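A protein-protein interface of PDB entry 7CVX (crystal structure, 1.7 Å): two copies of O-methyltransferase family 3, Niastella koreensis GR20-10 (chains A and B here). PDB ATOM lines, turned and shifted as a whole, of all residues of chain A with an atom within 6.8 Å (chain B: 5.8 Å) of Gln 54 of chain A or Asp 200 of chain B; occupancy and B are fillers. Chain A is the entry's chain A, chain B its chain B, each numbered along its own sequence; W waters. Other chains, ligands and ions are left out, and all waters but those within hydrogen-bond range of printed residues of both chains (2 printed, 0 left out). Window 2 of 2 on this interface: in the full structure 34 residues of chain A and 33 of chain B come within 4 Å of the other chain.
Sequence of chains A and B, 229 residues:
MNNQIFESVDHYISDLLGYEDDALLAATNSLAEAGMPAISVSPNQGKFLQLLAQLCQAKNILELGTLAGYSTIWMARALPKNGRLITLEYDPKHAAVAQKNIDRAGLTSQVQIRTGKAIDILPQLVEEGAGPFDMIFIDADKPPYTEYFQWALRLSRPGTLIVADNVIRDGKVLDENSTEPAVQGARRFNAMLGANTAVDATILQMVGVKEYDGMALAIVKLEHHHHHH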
ATOM      1  N   LEU A  17      -1.665  -2.243 -22.271  1.00  0.00           N
ATOM      2  CA  LEU A  17      -0.515  -2.613 -21.417  1.00  0.00           C
ATOM      3  C   LEU A  17       0.673  -3.167 -22.204  1.00  0.00           C
ATOM      4  O   LEU A  17       1.496  -3.791 -21.542  1.00  0.00           O
ATOM      5  CB  LEU A  17      -1.036  -3.687 -20.461  1.00  0.00           C
ATOM      6  CG  LEU A  17      -2.034  -3.168 -19.424  1.00  0.00           C
ATOM      7  CD1 LEU A  17      -2.701  -4.329 -18.690  1.00  0.00           C
ATOM      8  CD2 LEU A  17      -1.338  -2.249 -18.447  1.00  0.00           C
ATOM      9  N   LYS A  47       6.102  -8.444 -22.502  1.00  0.00           N
ATOM     10  CA  LYS A  47       5.802  -7.730 -21.251  1.00  0.00           C
ATOM     11  C   LYS A  47       5.766  -8.729 -20.083  1.00  0.00           C
ATOM     12  O   LYS A  47       6.235  -8.386 -19.007  1.00  0.00           O
ATOM     13  CB  LYS A  47       4.472  -6.995 -21.400  1.00  0.00           C
ATOM     14  CG  LYS A  47       4.072  -6.124 -20.214  1.00  0.00           C
ATOM     15  CD  LYS A  47       5.030  -4.965 -19.895  1.00  0.00           C
ATOM     16  CE  LYS A  47       4.433  -4.040 -18.846  1.00  0.00           C
ATOM     17  NZ  LYS A  47       3.336  -3.219 -19.403  1.00  0.00           N
ATOM     18  N   LEU A  49       7.406 -11.613 -19.731  1.00  0.00           N
ATOM     19  CA  LEU A  49       8.827 -11.988 -19.464  1.00  0.00           C
ATOM     20  C   LEU A  49       9.515 -10.835 -18.724  1.00  0.00           C
ATOM     21  O   LEU A  49      10.294 -11.122 -17.786  1.00  0.00           O
ATOM     22  CB  LEU A  49       9.544 -12.317 -20.777  1.00  0.00           C
ATOM     23  CG  LEU A  49       9.091 -13.625 -21.430  1.00  0.00           C
ATOM     24  CD1 LEU A  49       9.789 -13.788 -22.770  1.00  0.00           C
ATOM     25  CD2 LEU A  49       9.369 -14.834 -20.566  1.00  0.00           C
ATOM     26  N   GLN A  50       9.232  -9.597 -19.106  1.00  0.00           N
ATOM     27  CA  GLN A  50       9.817  -8.411 -18.438  1.00  0.00           C
ATOM     28  C   GLN A  50       9.345  -8.396 -16.974  1.00  0.00           C
ATOM     29  O   GLN A  50      10.216  -8.203 -16.067  1.00  0.00           O
ATOM     30  CB  GLN A  50       9.472  -7.142 -19.192  1.00  0.00           C
ATOM     31  CG  GLN A  50      10.160  -5.891 -18.623  1.00  0.00           C
ATOM     32  CD  GLN A  50       9.788  -4.672 -19.444  1.00  0.00           C
ATOM     33  OE1 GLN A  50       8.746  -4.054 -19.226  1.00  0.00           O
ATOM     34  NE2 GLN A  50      10.578  -4.382 -20.475  1.00  0.00           N
ATOM     35  N   LEU A  51       8.058  -8.572 -16.714  1.00  0.00           N
ATOM     36  CA  LEU A  51       7.526  -8.579 -15.320  1.00  0.00           C
ATOM     37  C   LEU A  51       8.139  -9.728 -14.499  1.00  0.00           C
ATOM     38  O   LEU A  51       8.446  -9.546 -13.295  1.00  0.00           O
ATOM     39  CB  LEU A  51       6.003  -8.697 -15.393  1.00  0.00           C
ATOM     40  CG  LEU A  51       5.282  -7.466 -15.941  1.00  0.00           C
ATOM     41  CD1 LEU A  51       3.812  -7.746 -16.179  1.00  0.00           C
ATOM     42  CD2 LEU A  51       5.435  -6.249 -15.056  1.00  0.00           C
ATOM     43  N   LEU A  52       8.301 -10.905 -15.079  1.00  0.00           N
ATOM     44  CA  LEU A  52       8.985 -12.017 -14.355  1.00  0.00           C
ATOM     45  C   LEU A  52      10.418 -11.606 -14.015  1.00  0.00           C
ATOM     46  O   LEU A  52      10.861 -11.933 -12.892  1.00  0.00           O
ATOM     47  CB  LEU A  52       8.961 -13.301 -15.181  1.00  0.00           C
ATOM     48  CG  LEU A  52       7.583 -13.912 -15.383  1.00  0.00           C
ATOM     49  CD1 LEU A  52       7.631 -14.994 -16.424  1.00  0.00           C
ATOM     50  CD2 LEU A  52       7.003 -14.454 -14.088  1.00  0.00           C
ATOM     51  N   ALA A  53      11.134 -10.944 -14.923  1.00  0.00           N
ATOM     52  CA  ALA A  53      12.521 -10.534 -14.640  1.00  0.00           C
ATOM     53  C   ALA A  53      12.504  -9.525 -13.493  1.00  0.00           C
ATOM     54  O   ALA A  53      13.390  -9.596 -12.645  1.00  0.00           O
ATOM     55  CB  ALA A  53      13.171 -10.002 -15.875  1.00  0.00           C
ATOM     56  N   GLN A  54      11.513  -8.648 -13.456  1.00  0.00           N
ATOM     57  CA  GLN A  54      11.403  -7.680 -12.336  1.00  0.00           C
ATOM     58  C   GLN A  54      11.100  -8.405 -11.021  1.00  0.00           C
ATOM     59  O   GLN A  54      11.675  -8.012  -9.988  1.00  0.00           O
ATOM     60  CB  GLN A  54      10.332  -6.621 -12.628  1.00  0.00           C
ATOM     61  CG  GLN A  54      10.636  -5.751 -13.817  1.00  0.00           C
ATOM     62  CD  GLN A  54       9.466  -4.815 -14.023  1.00  0.00           C
ATOM     63  OE1 GLN A  54       8.760  -4.886 -15.018  1.00  0.00           O
ATOM     64  NE2 GLN A  54       9.168  -4.020 -13.012  1.00  0.00           N
ATOM     65  N   LEU A  55      10.257  -9.428 -11.013  1.00  0.00           N
ATOM     66  CA  LEU A  55       9.922 -10.161  -9.759  1.00  0.00           C
ATOM     67  C   LEU A  55      11.158 -10.896  -9.245  1.00  0.00           C
ATOM     68  O   LEU A  55      11.338 -10.946  -8.023  1.00  0.00           O
ATOM     69  CB  LEU A  55       8.789 -11.173  -9.957  1.00  0.00           C
ATOM     70  CG  LEU A  55       7.364 -10.645 -10.106  1.00  0.00           C
ATOM     71  CD1 LEU A  55       6.401 -11.818 -10.292  1.00  0.00           C
ATOM     72  CD2 LEU A  55       6.923  -9.827  -8.900  1.00  0.00           C
ATOM     73  N   CYS A  56      12.013 -11.366 -10.151  1.00  0.00           N
ATOM     74  CA  CYS A  56      13.306 -12.055  -9.881  1.00  0.00           C
ATOM     75  C   CYS A  56      14.329 -11.027  -9.406  1.00  0.00           C
ATOM     76  O   CYS A  56      15.429 -11.436  -9.032  1.00  0.00           O
ATOM     77  CB  CYS A  56      13.818 -12.786 -11.129  1.00  0.00           C
ATOM     78  SG  CYS A  56      12.828 -14.256 -11.481  1.00  0.00           S
ATOM     79  N   GLN A  57      14.033  -9.736  -9.522  1.00  0.00           N
ATOM     80  CA  GLN A  57      15.029  -8.659  -9.332  1.00  0.00           C
ATOM     81  C   GLN A  57      16.298  -9.075 -10.073  1.00  0.00           C
ATOM     82  O   GLN A  57      17.429  -8.914  -9.548  1.00  0.00           O
ATOM     83  CB  GLN A  57      15.187  -8.433  -7.828  1.00  0.00           C
ATOM     84  CG  GLN A  57      13.928  -7.833  -7.225  1.00  0.00           C
ATOM     85  CD  GLN A  57      13.975  -7.823  -5.727  1.00  0.00           C
ATOM     86  OE1 GLN A  57      13.494  -8.746  -5.084  1.00  0.00           O
ATOM     87  NE2 GLN A  57      14.574  -6.773  -5.164  1.00  0.00           N
ATOM     88  N   ALA A  58      16.140  -9.533 -11.321  1.00  0.00           N
ATOM     89  CA  ALA A  58      17.231 -10.159 -12.086  1.00  0.00           C
ATOM     90  C   ALA A  58      18.364  -9.161 -12.334  1.00  0.00           C
ATOM     91  O   ALA A  58      18.116  -8.017 -12.742  1.00  0.00           O
ATOM     92  CB  ALA A  58      16.696 -10.700 -13.394  1.00  0.00           C
ATOM     93  N   MET A  75      13.367  -8.409 -21.926  1.00  0.00           N
ATOM     94  CA  MET A  75      13.979  -8.848 -20.643  1.00  0.00           C
ATOM     95  C   MET A  75      15.100  -7.911 -20.236  1.00  0.00           C
ATOM     96  O   MET A  75      15.209  -7.647 -19.039  1.00  0.00           O
ATOM     97  CB  MET A  75      14.504 -10.273 -20.720  1.00  0.00           C
ATOM     98  CG  MET A  75      13.334 -11.270 -20.803  1.00  0.00           C
ATOM     99  SD  MET A  75      13.905 -13.002 -20.751  1.00  0.00           S
ATOM    100  CE  MET A  75      14.603 -13.223 -22.381  1.00  0.00           C
ATOM    101  N   ARG A  77      15.507  -4.905 -20.637  1.00  0.00           N
ATOM    102  CA  ARG A  77      14.975  -3.618 -20.132  1.00  0.00           C
ATOM    103  C   ARG A  77      14.630  -3.710 -18.651  1.00  0.00           C
ATOM    104  O   ARG A  77      14.456  -2.644 -18.046  1.00  0.00           O
ATOM    105  CB  ARG A  77      13.847  -3.137 -21.030  1.00  0.00           C
ATOM    106  CG  ARG A  77      14.373  -2.438 -22.268  1.00  0.00           C
ATOM    107  CD  ARG A  77      13.306  -2.100 -23.289  1.00  0.00           C
ATOM    108  NE  ARG A  77      13.834  -1.255 -24.339  1.00  0.00           N
ATOM    109  CZ  ARG A  77      13.120  -0.853 -25.384  1.00  0.00           C
ATOM    110  NH1 ARG A  77      11.889  -1.307 -25.542  1.00  0.00           N
ATOM    111  NH2 ARG A  77      13.681  -0.112 -26.317  1.00  0.00           N
ATOM    112  N   ALA A  78      14.582  -4.903 -18.058  1.00  0.00           N
ATOM    113  CA  ALA A  78      14.275  -5.081 -16.631  1.00  0.00           C
ATOM    114  C   ALA A  78      15.561  -4.989 -15.842  1.00  0.00           C
ATOM    115  O   ALA A  78      15.458  -4.944 -14.649  1.00  0.00           O
ATOM    116  CB  ALA A  78      13.574  -6.384 -16.370  1.00  0.00           C
ATOM    117  N   LEU A  79      16.723  -4.981 -16.496  1.00  0.00           N
ATOM    118  CA  LEU A  79      17.997  -5.123 -15.765  1.00  0.00           C
ATOM    119  C   LEU A  79      18.373  -3.790 -15.127  1.00  0.00           C
ATOM    120  O   LEU A  79      18.138  -2.736 -15.713  1.00  0.00           O
ATOM    121  CB  LEU A  79      19.128  -5.514 -16.718  1.00  0.00           C
ATOM    122  CG  LEU A  79      19.040  -6.923 -17.300  1.00  0.00           C
ATOM    123  CD1 LEU A  79      19.998  -7.095 -18.465  1.00  0.00           C
ATOM    124  CD2 LEU A  79      19.324  -7.943 -16.221  1.00  0.00           C
ATOM    125  N   MET A 135      17.438 -15.621 -13.779  1.00  0.00           N
ATOM    126  CA  MET A 135      16.350 -16.087 -14.687  1.00  0.00           C
ATOM    127  C   MET A 135      16.988 -16.642 -15.958  1.00  0.00           C
ATOM    128  O   MET A 135      18.000 -16.065 -16.434  1.00  0.00           O
ATOM    129  CB  MET A 135      15.440 -14.921 -15.044  1.00  0.00           C
ATOM    130  CG  MET A 135      14.347 -15.241 -16.014  1.00  0.00           C
ATOM    131  SD  MET A 135      13.197 -13.796 -16.119  1.00  0.00           S
ATOM    132  CE  MET A 135      12.095 -14.394 -17.396  1.00  0.00           C
ATOM    133  N   ALA B 198       1.558   3.928 -11.298  1.00  0.00           N
ATOM    134  CA  ALA B 198       2.240   3.421 -10.089  1.00  0.00           C
ATOM    135  C   ALA B 198       2.701   1.976 -10.268  1.00  0.00           C
ATOM    136  O   ALA B 198       3.431   1.503  -9.392  1.00  0.00           O
ATOM    137  CB  ALA B 198       1.347   3.519  -8.876  1.00  0.00           C
ATOM    138  N   VAL B 199       2.243   1.289 -11.308  1.00  0.00           N
ATOM    139  CA  VAL B 199       2.546  -0.151 -11.502  1.00  0.00           C
ATOM    140  C   VAL B 199       3.019  -0.396 -12.935  1.00  0.00           C
ATOM    141  O   VAL B 199       2.611   0.365 -13.886  1.00  0.00           O
ATOM    142  CB  VAL B 199       1.341  -1.055 -11.195  1.00  0.00           C
ATOM    143  CG1 VAL B 199       0.816  -0.900  -9.776  1.00  0.00           C
ATOM    144  CG2 VAL B 199       0.225  -0.850 -12.182  1.00  0.00           C
ATOM    145  N   ASP B 200       3.781  -1.469 -13.083  1.00  0.00           N
ATOM    146  CA  ASP B 200       3.999  -2.162 -14.376  1.00  0.00           C
ATOM    147  C   ASP B 200       3.035  -3.362 -14.444  1.00  0.00           C
ATOM    148  O   ASP B 200       2.995  -4.137 -13.479  1.00  0.00           O
ATOM    149  CB  ASP B 200       5.469  -2.558 -14.522  1.00  0.00           C
ATOM    150  CG  ASP B 200       6.405  -1.355 -14.430  1.00  0.00           C
ATOM    151  OD1 ASP B 200       6.123  -0.354 -15.117  1.00  0.00           O
ATOM    152  OD2 ASP B 200       7.388  -1.414 -13.614  1.00  0.00           O
ATOM    153  N   ALA B 201       2.282  -3.523 -15.519  1.00  0.00           N
ATOM    154  CA  ALA B 201       1.205  -4.553 -15.548  1.00  0.00           C
ATOM    155  C   ALA B 201       1.011  -5.237 -16.904  1.00  0.00           C
ATOM    156  O   ALA B 201       1.437  -4.735 -17.967  1.00  0.00           O
ATOM    157  CB  ALA B 201      -0.089  -3.959 -15.063  1.00  0.00           C
ATOM    158  N   THR B 202       0.361  -6.394 -16.836  1.00  0.00           N
ATOM    159  CA  THR B 202      -0.088  -7.160 -18.015  1.00  0.00           C
ATOM    160  C   THR B 202      -1.366  -7.882 -17.631  1.00  0.00           C
ATOM    161  O   THR B 202      -1.768  -7.924 -16.426  1.00  0.00           O
ATOM    162  CB  THR B 202       0.966  -8.104 -18.616  1.00  0.00           C
ATOM    163  OG1 THR B 202       0.536  -8.375 -19.953  1.00  0.00           O
ATOM    164  CG2 THR B 202       1.217  -9.389 -17.847  1.00  0.00           C
ATOM    165  N   LEU B 217      -1.729  -9.045 -13.707  1.00  0.00           N
ATOM    166  CA  LEU B 217      -0.516  -9.071 -12.860  1.00  0.00           C
ATOM    167  C   LEU B 217       0.044  -7.653 -12.883  1.00  0.00           C
ATOM    168  O   LEU B 217       0.230  -7.086 -13.984  1.00  0.00           O
ATOM    169  CB  LEU B 217       0.532 -10.062 -13.407  1.00  0.00           C
ATOM    170  CG  LEU B 217       0.194 -11.544 -13.599  1.00  0.00           C
ATOM    171  CD1 LEU B 217       1.446 -12.302 -14.020  1.00  0.00           C
ATOM    172  CD2 LEU B 217      -0.354 -12.187 -12.358  1.00  0.00           C
ATOM    173  N   ALA B 218       0.306  -7.064 -11.727  1.00  0.00           N
ATOM    174  CA  ALA B 218       0.850  -5.708 -11.618  1.00  0.00           C
ATOM    175  C   ALA B 218       1.946  -5.685 -10.574  1.00  0.00           C
ATOM    176  O   ALA B 218       1.715  -6.223  -9.507  1.00  0.00           O
ATOM    177  CB  ALA B 218      -0.256  -4.769 -11.248  1.00  0.00           C
ATOM    178  N   ILE B 219       3.084  -5.054 -10.865  1.00  0.00           N
ATOM    179  CA  ILE B 219       4.165  -4.880  -9.857  1.00  0.00           C
ATOM    180  C   ILE B 219       4.346  -3.384  -9.563  1.00  0.00           C
ATOM    181  O   ILE B 219       4.501  -2.545 -10.498  1.00  0.00           O
ATOM    182  CB  ILE B 219       5.485  -5.504 -10.334  1.00  0.00           C
ATOM    183  CG1 ILE B 219       5.291  -6.947 -10.754  1.00  0.00           C
ATOM    184  CG2 ILE B 219       6.539  -5.319  -9.252  1.00  0.00           C
ATOM    185  CD1 ILE B 219       6.473  -7.525 -11.468  1.00  0.00           C
ATOM    186  N   VAL B 220       4.301  -3.059  -8.268  1.00  0.00           N
ATOM    187  CA  VAL B 220       4.362  -1.654  -7.801  1.00  0.00           C
ATOM    188  C   VAL B 220       5.799  -1.189  -8.051  1.00  0.00           C
ATOM    189  O   VAL B 220       6.738  -1.941  -7.739  1.00  0.00           O
ATOM    190  CB  VAL B 220       3.906  -1.585  -6.335  1.00  0.00           C
ATOM    191  CG1 VAL B 220       4.025  -0.171  -5.786  1.00  0.00           C
ATOM    192  CG2 VAL B 220       2.480  -2.117  -6.223  1.00  0.00           C
ATOM    193  N   LYS B 221       5.969  -0.079  -8.755  1.00  0.00           N
ATOM    194  CA  LYS B 221       7.306   0.352  -9.249  1.00  0.00           C
ATOM    195  C   LYS B 221       8.246   0.676  -8.074  1.00  0.00           C
ATOM    196  O   LYS B 221       7.744   1.050  -6.986  1.00  0.00           O
ATOM    197  CB  LYS B 221       7.147   1.575 -10.147  1.00  0.00           C
ATOM    198  CG  LYS B 221       6.295   1.372 -11.383  1.00  0.00           C
ATOM    199  CD  LYS B 221       6.098   2.680 -12.133  1.00  0.00           C
ATOM    200  CE  LYS B 221       5.490   2.500 -13.507  1.00  0.00           C
ATOM    201  NZ  LYS B 221       5.548   3.745 -14.292  1.00  0.00           N
HETATM  202  O   HOH W   1       0.980  -6.661 -21.890  1.00  0.00           O
HETATM  203  O   HOH W   2       2.115  -1.253 -17.231  1.00  0.00           O
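The side-chain amino group (NZ) of Lys 47 of chain A sits at hydrogen-bond distance from the backbone carbonyl oxygen (O) of Ala 201 of chain B (2.8 Å). The side-chain carboxylate (OD2) of Asp 200 of chain B sits at hydrogen-bond distance from the side-chain amide nitrogen (NE2) of Gln 54 of chain A (3.2 Å).
The backbone carbonyl oxygen (O) of Leu 17 of chain A sits at hydrogen-bond distance from the side-chain amino group (NZ) of Lys 47 of chain A, 2.9 Å away. The backbone NH of Ile 219 of chain B lies within hydrogen-bond range of the backbone carbonyl oxygen of Asp 200 of chain B (2.8 Å). The backbone NH (N) of Thr 202 of chain B sits at hydrogen-bond distance from the backbone carbonyl oxygen (O) of Leu 217 of chain B (2.9 Å).
Among the printed residues, merely in contact across the chains: Leu 51 of chain A with Ile 219 of chain B, Leu 55 of chain A with Ile 219 of chain B, Leu 51 of chain A with Thr 202 of chain B, Leu 51 of chain A with Asp 200 of chain B, Leu 17 of chain A with Ala 201 of chain B, Leu 51 of chain A with Ala 201 of chain B and Leu 17 of chain A with Thr 202 of chain B.
Gln 54 of chain A touches just one residue of chain B: Asp 200 (3.2 Å). Asp 200 of chain B touches just these residues of chain A: Leu 51 and Gln 54. Printed residues of chain B within 4 Å of Lys 47 of chain A: Ala 201. Printed residues of chain A within 4 Å of Ile 219 of chain B: Leu 51 (3.4 Å) and Leu 55 (3.5 Å). Printed residues of chain B within 4 Å of Leu 51 of chain A: Asp 200 (3.6 Å), Ala 201 (3.8 Å), Thr 202 (3.5 Å) and Ile 219 (3.4 Å). Of the printed residues of chain A, Ala 201 of chain B touches Leu 17, Lys 47 and Leu 51. Of the printed residues of chain B, Leu 17 of chain A touches Ala 201 (3.7 Å) and Thr 202 (3.9 Å). Met 135 of chain A touches none of the printed residues of chain B. The nearest printed residue of chain B that does not touch Lys 47 of chain A is Thr 202 of chain B (4.02 Å).
Hydrophobic or aromatic side chains of chain A within 4 Å of the printed part of chain B: Leu 17, Leu 51 and Leu 55. Hydrophobic or aromatic side chains of chain B that line the printed part of chain A: Ala 201 and Ile 219. Among the printed residues, 9 pairs touch across the chains.
No position is printed for both chains.
Water W1 bridges OG1 of Thr 202 of chain B (2.6 Å) and O of Leu 17 of chain A (2.9 Å). Water W2 bridges the backbone NH (N) of Ala 201 of chain B (2.8 Å) and the side-chain amino group (NZ) of Lys 47 of chain A (3.2 Å).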
